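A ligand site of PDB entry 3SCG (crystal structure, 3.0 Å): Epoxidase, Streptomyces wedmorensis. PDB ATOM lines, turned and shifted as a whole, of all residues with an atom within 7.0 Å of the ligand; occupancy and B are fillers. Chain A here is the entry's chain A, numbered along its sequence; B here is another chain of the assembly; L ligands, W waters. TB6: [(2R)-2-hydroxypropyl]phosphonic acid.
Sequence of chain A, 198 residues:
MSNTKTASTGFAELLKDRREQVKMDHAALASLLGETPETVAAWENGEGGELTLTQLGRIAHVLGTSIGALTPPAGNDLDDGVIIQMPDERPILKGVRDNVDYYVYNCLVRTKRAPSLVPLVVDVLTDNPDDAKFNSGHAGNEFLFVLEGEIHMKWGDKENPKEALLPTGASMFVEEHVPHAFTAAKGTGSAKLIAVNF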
ATOM      1  N   ARG A  97     -24.434   9.020  -1.140  1.00  0.00           N
ATOM      2  CA  ARG A  97     -25.746   9.581  -0.830  1.00  0.00           C
ATOM      3  C   ARG A  97     -26.850   8.727  -1.442  1.00  0.00           C
ATOM      4  O   ARG A  97     -26.991   8.682  -2.665  1.00  0.00           O
ATOM      5  CB  ARG A  97     -25.864  11.006  -1.358  1.00  0.00           C
ATOM      6  CG  ARG A  97     -24.839  11.958  -0.785  1.00  0.00           C
ATOM      7  CD  ARG A  97     -25.078  13.373  -1.237  1.00  0.00           C
ATOM      8  NE  ARG A  97     -24.029  14.262  -0.751  1.00  0.00           N
ATOM      9  CZ  ARG A  97     -23.984  15.566  -0.988  1.00  0.00           C
ATOM     10  NH1 ARG A  97     -24.927  16.160  -1.704  1.00  0.00           N
ATOM     11  NH2 ARG A  97     -22.978  16.281  -0.494  1.00  0.00           N
ATOM     12  N   TYR A 102     -21.285   9.642  -4.711  1.00  0.00           N
ATOM     13  CA  TYR A 102     -21.545  10.945  -5.297  1.00  0.00           C
ATOM     14  C   TYR A 102     -20.281  11.778  -5.476  1.00  0.00           C
ATOM     15  O   TYR A 102     -20.109  12.428  -6.513  1.00  0.00           O
ATOM     16  CB  TYR A 102     -22.557  11.694  -4.426  1.00  0.00           C
ATOM     17  CG  TYR A 102     -23.437  12.619  -5.217  1.00  0.00           C
ATOM     18  CD1 TYR A 102     -24.465  12.118  -6.025  1.00  0.00           C
ATOM     19  CD2 TYR A 102     -23.221  13.990  -5.206  1.00  0.00           C
ATOM     20  CE1 TYR A 102     -25.255  12.971  -6.790  1.00  0.00           C
ATOM     21  CE2 TYR A 102     -23.998  14.847  -5.969  1.00  0.00           C
ATOM     22  CZ  TYR A 102     -25.019  14.337  -6.755  1.00  0.00           C
ATOM     23  OH  TYR A 102     -25.794  15.200  -7.497  1.00  0.00           O
ATOM     24  N   TYR A 103     -19.425  11.778  -4.462  1.00  0.00           N
ATOM     25  CA  TYR A 103     -18.172  12.539  -4.503  1.00  0.00           C
ATOM     26  C   TYR A 103     -17.039  11.741  -3.878  1.00  0.00           C
ATOM     27  O   TYR A 103     -17.245  10.675  -3.291  1.00  0.00           O
ATOM     28  CB  TYR A 103     -18.263  13.838  -3.690  1.00  0.00           C
ATOM     29  CG  TYR A 103     -19.386  14.802  -4.023  1.00  0.00           C
ATOM     30  CD1 TYR A 103     -19.657  15.178  -5.333  1.00  0.00           C
ATOM     31  CD2 TYR A 103     -20.140  15.386  -3.000  1.00  0.00           C
ATOM     32  CE1 TYR A 103     -20.646  16.119  -5.631  1.00  0.00           C
ATOM     33  CE2 TYR A 103     -21.131  16.332  -3.289  1.00  0.00           C
ATOM     34  CZ  TYR A 103     -21.382  16.690  -4.605  1.00  0.00           C
ATOM     35  OH  TYR A 103     -22.372  17.607  -4.900  1.00  0.00           O
ATOM     36  N   TYR A 105     -13.647  13.164  -1.706  1.00  0.00           N
ATOM     37  CA  TYR A 105     -13.040  14.373  -1.190  1.00  0.00           C
ATOM     38  C   TYR A 105     -11.545  14.276  -1.040  1.00  0.00           C
ATOM     39  O   TYR A 105     -11.056  13.494  -0.238  1.00  0.00           O
ATOM     40  CB  TYR A 105     -13.663  14.689   0.157  1.00  0.00           C
ATOM     41  CG  TYR A 105     -15.121  15.053   0.061  1.00  0.00           C
ATOM     42  CD1 TYR A 105     -15.513  16.294  -0.431  1.00  0.00           C
ATOM     43  CD2 TYR A 105     -16.108  14.168   0.491  1.00  0.00           C
ATOM     44  CE1 TYR A 105     -16.845  16.657  -0.483  1.00  0.00           C
ATOM     45  CE2 TYR A 105     -17.450  14.522   0.429  1.00  0.00           C
ATOM     46  CZ  TYR A 105     -17.808  15.766  -0.055  1.00  0.00           C
ATOM     47  OH  TYR A 105     -19.131  16.143  -0.088  1.00  0.00           O
ATOM     48  N   LEU A 120     -10.608  21.716  -0.793  1.00  0.00           N
ATOM     49  CA  LEU A 120     -10.747  20.342  -1.256  1.00  0.00           C
ATOM     50  C   LEU A 120     -10.669  20.237  -2.760  1.00  0.00           C
ATOM     51  O   LEU A 120     -10.778  21.231  -3.480  1.00  0.00           O
ATOM     52  CB  LEU A 120     -12.111  19.778  -0.837  1.00  0.00           C
ATOM     53  CG  LEU A 120     -12.580  19.884   0.608  1.00  0.00           C
ATOM     54  CD1 LEU A 120     -14.089  19.758   0.642  1.00  0.00           C
ATOM     55  CD2 LEU A 120     -11.921  18.807   1.456  1.00  0.00           C
ATOM     56  N   VAL A 122     -12.710  18.038  -5.252  1.00  0.00           N
ATOM     57  CA  VAL A 122     -13.839  17.132  -5.275  1.00  0.00           C
ATOM     58  C   VAL A 122     -14.069  16.466  -6.630  1.00  0.00           C
ATOM     59  O   VAL A 122     -14.140  17.133  -7.661  1.00  0.00           O
ATOM     60  CB  VAL A 122     -15.131  17.858  -4.866  1.00  0.00           C
ATOM     61  CG1 VAL A 122     -16.277  16.873  -4.748  1.00  0.00           C
ATOM     62  CG2 VAL A 122     -14.925  18.590  -3.561  1.00  0.00           C
ATOM     63  N   VAL A 124     -16.576  14.840  -8.878  1.00  0.00           N
ATOM     64  CA  VAL A 124     -18.010  14.716  -9.114  1.00  0.00           C
ATOM     65  C   VAL A 124     -18.227  13.403  -9.887  1.00  0.00           C
ATOM     66  O   VAL A 124     -18.054  13.356 -11.113  1.00  0.00           O
ATOM     67  CB  VAL A 124     -18.526  15.921  -9.921  1.00  0.00           C
ATOM     68  CG1 VAL A 124     -20.034  15.883 -10.039  1.00  0.00           C
ATOM     69  CG2 VAL A 124     -18.069  17.206  -9.258  1.00  0.00           C
ATOM     70  N   LYS A 133     -28.085  15.073  -5.885  1.00  0.00           N
ATOM     71  CA  LYS A 133     -28.335  14.928  -4.455  1.00  0.00           C
ATOM     72  C   LYS A 133     -27.919  16.183  -3.713  1.00  0.00           C
ATOM     73  O   LYS A 133     -26.731  16.425  -3.487  1.00  0.00           O
ATOM     74  CB  LYS A 133     -27.565  13.719  -3.916  1.00  0.00           C
ATOM     75  CG  LYS A 133     -27.859  12.408  -4.630  1.00  0.00           C
ATOM     76  CD  LYS A 133     -29.327  12.042  -4.529  1.00  0.00           C
ATOM     77  CE  LYS A 133     -29.628  10.710  -5.208  1.00  0.00           C
ATOM     78  NZ  LYS A 133     -31.067  10.357  -5.082  1.00  0.00           N
ATOM     79  N   PHE A 134     -28.907  16.981  -3.332  1.00  0.00           N
ATOM     80  CA  PHE A 134     -28.673  18.234  -2.613  1.00  0.00           C
ATOM     81  C   PHE A 134     -28.188  18.041  -1.187  1.00  0.00           C
ATOM     82  O   PHE A 134     -28.514  17.048  -0.540  1.00  0.00           O
ATOM     83  CB  PHE A 134     -29.968  19.054  -2.522  1.00  0.00           C
ATOM     84  CG  PHE A 134     -30.241  19.925  -3.700  1.00  0.00           C
ATOM     85  CD1 PHE A 134     -30.646  19.376  -4.917  1.00  0.00           C
ATOM     86  CD2 PHE A 134     -30.147  21.303  -3.599  1.00  0.00           C
ATOM     87  CE1 PHE A 134     -30.951  20.200  -6.004  1.00  0.00           C
ATOM     88  CE2 PHE A 134     -30.450  22.134  -4.664  1.00  0.00           C
ATOM     89  CZ  PHE A 134     -30.860  21.578  -5.878  1.00  0.00           C
ATOM     90  N   ASN A 135     -27.390  18.992  -0.727  1.00  0.00           N
ATOM     91  CA  ASN A 135     -26.926  18.980   0.653  1.00  0.00           C
ATOM     92  C   ASN A 135     -27.972  19.908   1.301  1.00  0.00           C
ATOM     93  O   ASN A 135     -28.927  20.307   0.630  1.00  0.00           O
ATOM     94  CB  ASN A 135     -25.509  19.544   0.804  1.00  0.00           C
ATOM     95  CG  ASN A 135     -25.348  20.963   0.264  1.00  0.00           C
ATOM     96  OD1 ASN A 135     -26.324  21.695   0.101  1.00  0.00           O
ATOM     97  ND2 ASN A 135     -24.100  21.361   0.007  1.00  0.00           N
ATOM     98  N   SER A 136     -27.806  20.240   2.573  1.00  0.00           N
ATOM     99  CA  SER A 136     -28.777  21.111   3.221  1.00  0.00           C
ATOM    100  C   SER A 136     -28.224  22.509   3.392  1.00  0.00           C
ATOM    101  O   SER A 136     -28.792  23.341   4.090  1.00  0.00           O
ATOM    102  CB  SER A 136     -29.151  20.538   4.583  1.00  0.00           C
ATOM    103  OG  SER A 136     -29.602  19.198   4.460  1.00  0.00           O
ATOM    104  N   GLY A 137     -27.108  22.774   2.719  1.00  0.00           N
ATOM    105  CA  GLY A 137     -26.457  24.055   2.849  1.00  0.00           C
ATOM    106  C   GLY A 137     -25.492  23.850   3.992  1.00  0.00           C
ATOM    107  O   GLY A 137     -25.570  22.829   4.679  1.00  0.00           O
ATOM    108  N   HIS A 138     -24.564  24.781   4.201  1.00  0.00           N
ATOM    109  CA  HIS A 138     -23.624  24.617   5.297  1.00  0.00           C
ATOM    110  C   HIS A 138     -22.996  25.936   5.727  1.00  0.00           C
ATOM    111  O   HIS A 138     -22.819  26.854   4.930  1.00  0.00           O
ATOM    112  CB  HIS A 138     -22.537  23.589   4.923  1.00  0.00           C
ATOM    113  CG  HIS A 138     -21.874  23.840   3.602  1.00  0.00           C
ATOM    114  ND1 HIS A 138     -21.187  24.994   3.283  1.00  0.00           N
ATOM    115  CD2 HIS A 138     -21.761  23.037   2.510  1.00  0.00           C
ATOM    116  CE1 HIS A 138     -20.682  24.848   2.048  1.00  0.00           C
ATOM    117  NE2 HIS A 138     -21.014  23.685   1.547  1.00  0.00           N
ATOM    118  N   GLU A 142     -18.489  29.502   0.378  1.00  0.00           N
ATOM    119  CA  GLU A 142     -17.659  28.575  -0.356  1.00  0.00           C
ATOM    120  C   GLU A 142     -17.301  29.103  -1.732  1.00  0.00           C
ATOM    121  O   GLU A 142     -18.141  29.647  -2.443  1.00  0.00           O
ATOM    122  CB  GLU A 142     -18.384  27.250  -0.508  1.00  0.00           C
ATOM    123  CG  GLU A 142     -17.556  26.122  -1.080  1.00  0.00           C
ATOM    124  CD  GLU A 142     -18.409  24.926  -1.430  1.00  0.00           C
ATOM    125  OE1 GLU A 142     -19.494  24.754  -0.830  1.00  0.00           O
ATOM    126  OE2 GLU A 142     -18.004  24.147  -2.314  1.00  0.00           O
ATOM    127  N   LEU A 144     -15.790  28.020  -5.453  1.00  0.00           N
ATOM    128  CA  LEU A 144     -15.531  26.840  -6.271  1.00  0.00           C
ATOM    129  C   LEU A 144     -14.872  27.187  -7.591  1.00  0.00           C
ATOM    130  O   LEU A 144     -14.938  28.315  -8.074  1.00  0.00           O
ATOM    131  CB  LEU A 144     -16.829  26.077  -6.539  1.00  0.00           C
ATOM    132  CG  LEU A 144     -17.614  25.577  -5.325  1.00  0.00           C
ATOM    133  CD1 LEU A 144     -18.971  26.273  -5.275  1.00  0.00           C
ATOM    134  CD2 LEU A 144     -17.778  24.071  -5.419  1.00  0.00           C
ATOM    135  N   HIS A 180     -26.913  23.192  -2.227  1.00  0.00           N
ATOM    136  CA  HIS A 180     -26.406  23.036  -3.590  1.00  0.00           C
ATOM    137  C   HIS A 180     -26.029  21.587  -3.905  1.00  0.00           C
ATOM    138  O   HIS A 180     -25.834  20.764  -3.005  1.00  0.00           O
ATOM    139  CB  HIS A 180     -25.195  23.950  -3.802  1.00  0.00           C
ATOM    140  CG  HIS A 180     -24.239  23.963  -2.652  1.00  0.00           C
ATOM    141  ND1 HIS A 180     -24.552  24.427  -1.404  1.00  0.00           N
ATOM    142  CD2 HIS A 180     -22.961  23.507  -2.573  1.00  0.00           C
ATOM    143  CE1 HIS A 180     -23.488  24.230  -0.601  1.00  0.00           C
ATOM    144  NE2 HIS A 180     -22.499  23.681  -1.261  1.00  0.00           N
ATOM    145  N   ALA A 181     -25.936  21.273  -5.199  1.00  0.00           N
ATOM    146  CA  ALA A 181     -25.582  19.934  -5.652  1.00  0.00           C
ATOM    147  C   ALA A 181     -24.863  20.046  -6.989  1.00  0.00           C
ATOM    148  O   ALA A 181     -25.074  21.000  -7.744  1.00  0.00           O
ATOM    149  CB  ALA A 181     -26.830  19.075  -5.794  1.00  0.00           C
ATOM    150  N   PHE A 182     -24.021  19.050  -7.283  1.00  0.00           N
ATOM    151  CA  PHE A 182     -23.255  19.017  -8.526  1.00  0.00           C
ATOM    152  C   PHE A 182     -23.265  17.609  -9.133  1.00  0.00           C
ATOM    153  O   PHE A 182     -23.466  16.620  -8.434  1.00  0.00           O
ATOM    154  CB  PHE A 182     -21.805  19.415  -8.260  1.00  0.00           C
ATOM    155  CG  PHE A 182     -21.623  20.793  -7.699  1.00  0.00           C
ATOM    156  CD1 PHE A 182     -21.776  21.919  -8.505  1.00  0.00           C
ATOM    157  CD2 PHE A 182     -21.349  20.980  -6.349  1.00  0.00           C
ATOM    158  CE1 PHE A 182     -21.651  23.198  -7.975  1.00  0.00           C
ATOM    159  CE2 PHE A 182     -21.230  22.251  -5.816  1.00  0.00           C
ATOM    160  CZ  PHE A 182     -21.378  23.368  -6.638  1.00  0.00           C
ATOM    161  N   LEU A 193     -14.099  19.502  -9.414  1.00  0.00           N
ATOM    162  CA  LEU A 193     -14.146  20.822  -8.808  1.00  0.00           C
ATOM    163  C   LEU A 193     -13.051  20.972  -7.783  1.00  0.00           C
ATOM    164  O   LEU A 193     -12.382  20.013  -7.410  1.00  0.00           O
ATOM    165  CB  LEU A 193     -15.458  21.034  -8.059  1.00  0.00           C
ATOM    166  CG  LEU A 193     -16.789  21.293  -8.745  1.00  0.00           C
ATOM    167  CD1 LEU A 193     -17.889  21.259  -7.697  1.00  0.00           C
ATOM    168  CD2 LEU A 193     -16.751  22.638  -9.452  1.00  0.00           C
ATOM    169  N   ILE A 194     -12.877  22.199  -7.327  1.00  0.00           N
ATOM    170  CA  ILE A 194     -11.950  22.470  -6.249  1.00  0.00           C
ATOM    171  C   ILE A 194     -12.714  23.443  -5.362  1.00  0.00           C
ATOM    172  O   ILE A 194     -12.851  24.614  -5.663  1.00  0.00           O
ATOM    173  CB  ILE A 194     -10.571  23.022  -6.742  1.00  0.00           C
ATOM    174  CG1 ILE A 194      -9.945  23.849  -5.625  1.00  0.00           C
ATOM    175  CG2 ILE A 194     -10.722  23.784  -8.032  1.00  0.00           C
ATOM    176  CD1 ILE A 194      -8.531  24.221  -5.895  1.00  0.00           C
ATOM    177  N   ALA A 195     -13.263  22.897  -4.285  1.00  0.00           N
ATOM    178  CA  ALA A 195     -14.059  23.663  -3.352  1.00  0.00           C
ATOM    179  C   ALA A 195     -13.239  24.226  -2.200  1.00  0.00           C
ATOM    180  O   ALA A 195     -12.358  23.551  -1.651  1.00  0.00           O
ATOM    181  CB  ALA A 195     -15.173  22.788  -2.801  1.00  0.00           C
ATOM    182  N   VAL A 196     -13.544  25.460  -1.824  1.00  0.00           N
ATOM    183  CA  VAL A 196     -12.858  26.106  -0.720  1.00  0.00           C
ATOM    184  C   VAL A 196     -13.878  26.690   0.251  1.00  0.00           C
ATOM    185  O   VAL A 196     -14.597  27.628  -0.102  1.00  0.00           O
ATOM    186  CB  VAL A 196     -11.965  27.254  -1.199  1.00  0.00           C
ATOM    187  CG1 VAL A 196     -11.295  27.907  -0.006  1.00  0.00           C
ATOM    188  CG2 VAL A 196     -10.927  26.718  -2.181  1.00  0.00           C
ATOM    189  N   ASN A 197     -13.956  26.116   1.443  1.00  0.00           N
ATOM    190  CA  ASN A 197     -14.864  26.610   2.471  1.00  0.00           C
ATOM    191  C   ASN A 197     -14.041  27.440   3.432  1.00  0.00           C
ATOM    192  O   ASN A 197     -13.133  26.927   4.086  1.00  0.00           O
ATOM    193  CB  ASN A 197     -15.498  25.452   3.240  1.00  0.00           C
ATOM    194  CG  ASN A 197     -16.405  24.602   2.373  1.00  0.00           C
ATOM    195  OD1 ASN A 197     -17.536  24.989   2.055  1.00  0.00           O
ATOM    196  ND2 ASN A 197     -15.898  23.437   1.961  1.00  0.00           N
ATOM    197  N   LYS B  23     -14.444  16.742   6.512  1.00  0.00           N
ATOM    198  CA  LYS B  23     -14.626  15.536   5.709  1.00  0.00           C
ATOM    199  C   LYS B  23     -14.009  14.272   6.279  1.00  0.00           C
ATOM    200  O   LYS B  23     -13.154  13.650   5.645  1.00  0.00           O
ATOM    201  CB  LYS B  23     -14.112  15.772   4.286  1.00  0.00           C
ATOM    202  CG  LYS B  23     -14.845  16.862   3.539  1.00  0.00           C
ATOM    203  CD  LYS B  23     -16.324  16.578   3.523  1.00  0.00           C
ATOM    204  CE  LYS B  23     -17.129  17.804   3.170  1.00  0.00           C
ATOM    205  NZ  LYS B  23     -18.586  17.536   3.312  1.00  0.00           N
HETATM  206  C1  TB6 L   1     -18.642  20.846  -3.740  1.00  0.00           C
HETATM  207  C2  TB6 L   1     -19.127  20.588  -2.319  1.00  0.00           C
HETATM  208  C6  TB6 L   1     -20.463  19.834  -2.286  1.00  0.00           C
HETATM  209  P7  TB6 L   1     -20.986  19.560  -0.561  1.00  0.00           P
HETATM  210  O10 TB6 L   1     -19.282  21.829  -1.651  1.00  0.00           O
HETATM  211  O12 TB6 L   1     -22.250  18.855  -0.461  1.00  0.00           O
HETATM  212  O13 TB6 L   1     -21.033  20.938   0.168  1.00  0.00           O
HETATM  213  O14 TB6 L   1     -19.829  18.898   0.270  1.00  0.00           O
HETATM  214  O   HOH W   1     -24.170  18.833  -2.901  1.00  0.00           O
HETATM  215  O   HOH W   2     -18.295  22.748   0.808  1.00  0.00           O
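Water W2 lies within hydrogen-bond range of OD1 of Asn 197 (2.7 Å), O10 of the ligand (2.8 Å), OE1 of Glu 142 (2.9 Å) and NE2 of His 138 (3.0 Å). Water W1 lies within hydrogen-bond range of O of His 180, OH of Tyr 103, NH1 of Arg 97 and O12 of the ligand.
The side-chain hydroxyl (OH) of Tyr 105 is in hydrogen-bond range of an oxygen (O14) of the ligand (2.9 Å). NE2 of His 180 sits at hydrogen-bond distance from O13 of the ligand, at 3.4 Å. An oxygen (O10) of the ligand sits at hydrogen-bond distance from the side-chain carboxylate (OE2) of Glu 142. The side-chain amide nitrogen (ND2) of Asn 135 is in hydrogen-bond range of an oxygen (O13) of the ligand, 3.1 Å away. An oxygen (O12) of the ligand lies within salt-bridge range of the guanidinium group (NH2) of Arg 97 (2.7 Å). NZ of Lys 23 of chain B lies within salt-bridge range of O14 of the ligand. A ring nitrogen (NE2) of His 138 is in hydrogen-bond range of an oxygen (O13) of the ligand (3.1 Å).
The side-chain amide oxygen (OD1) of Asn 135 lies within hydrogen-bond range of the backbone NH (N) of Gly 137 (2.9 Å). The side-chain amide oxygen (OD1) of Asn 135 lies within hydrogen-bond range of the backbone NH (N) of His 180 (2.8 Å). The side-chain hydroxyl (OH) of Tyr 102 sits at hydrogen-bond distance from the backbone carbonyl oxygen (O) of Phe 182 (2.9 Å). A ring nitrogen (NE2) of His 138 sits at hydrogen-bond distance from the side-chain carboxylate (OE1) of Glu 142 (3.0 Å). The backbone NH (N) of Phe 182 is in hydrogen-bond range of the side-chain hydroxyl (OH) of Tyr 103, 3.2 Å away. NE2 of His 180 is in hydrogen-bond range of NE2 of His 138. The side-chain carboxylate (OE1) of Glu 142 lies within hydrogen-bond range of a ring nitrogen (NE2) of His 180. NH1 of Arg 97 is in hydrogen-bond range of O of Lys 133 (2.6 Å).
Residues that only touch the ligand: Tyr 103, Leu 144 and Phe 182. Hydrophobic or aromatic side chains within 4 Å of the ligand: Tyr 103, Tyr 105, His 138, Leu 144 and Phe 182. Within 4 Å of the ligand: Arg 97, Tyr 103, Tyr 105, Asn 135, His 138, Glu 142, Leu 144, His 180, Phe 182 and Lys 23 of chain B. The nearest printed residue that does not touch the ligand is Leu 193 (4.05 Å).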
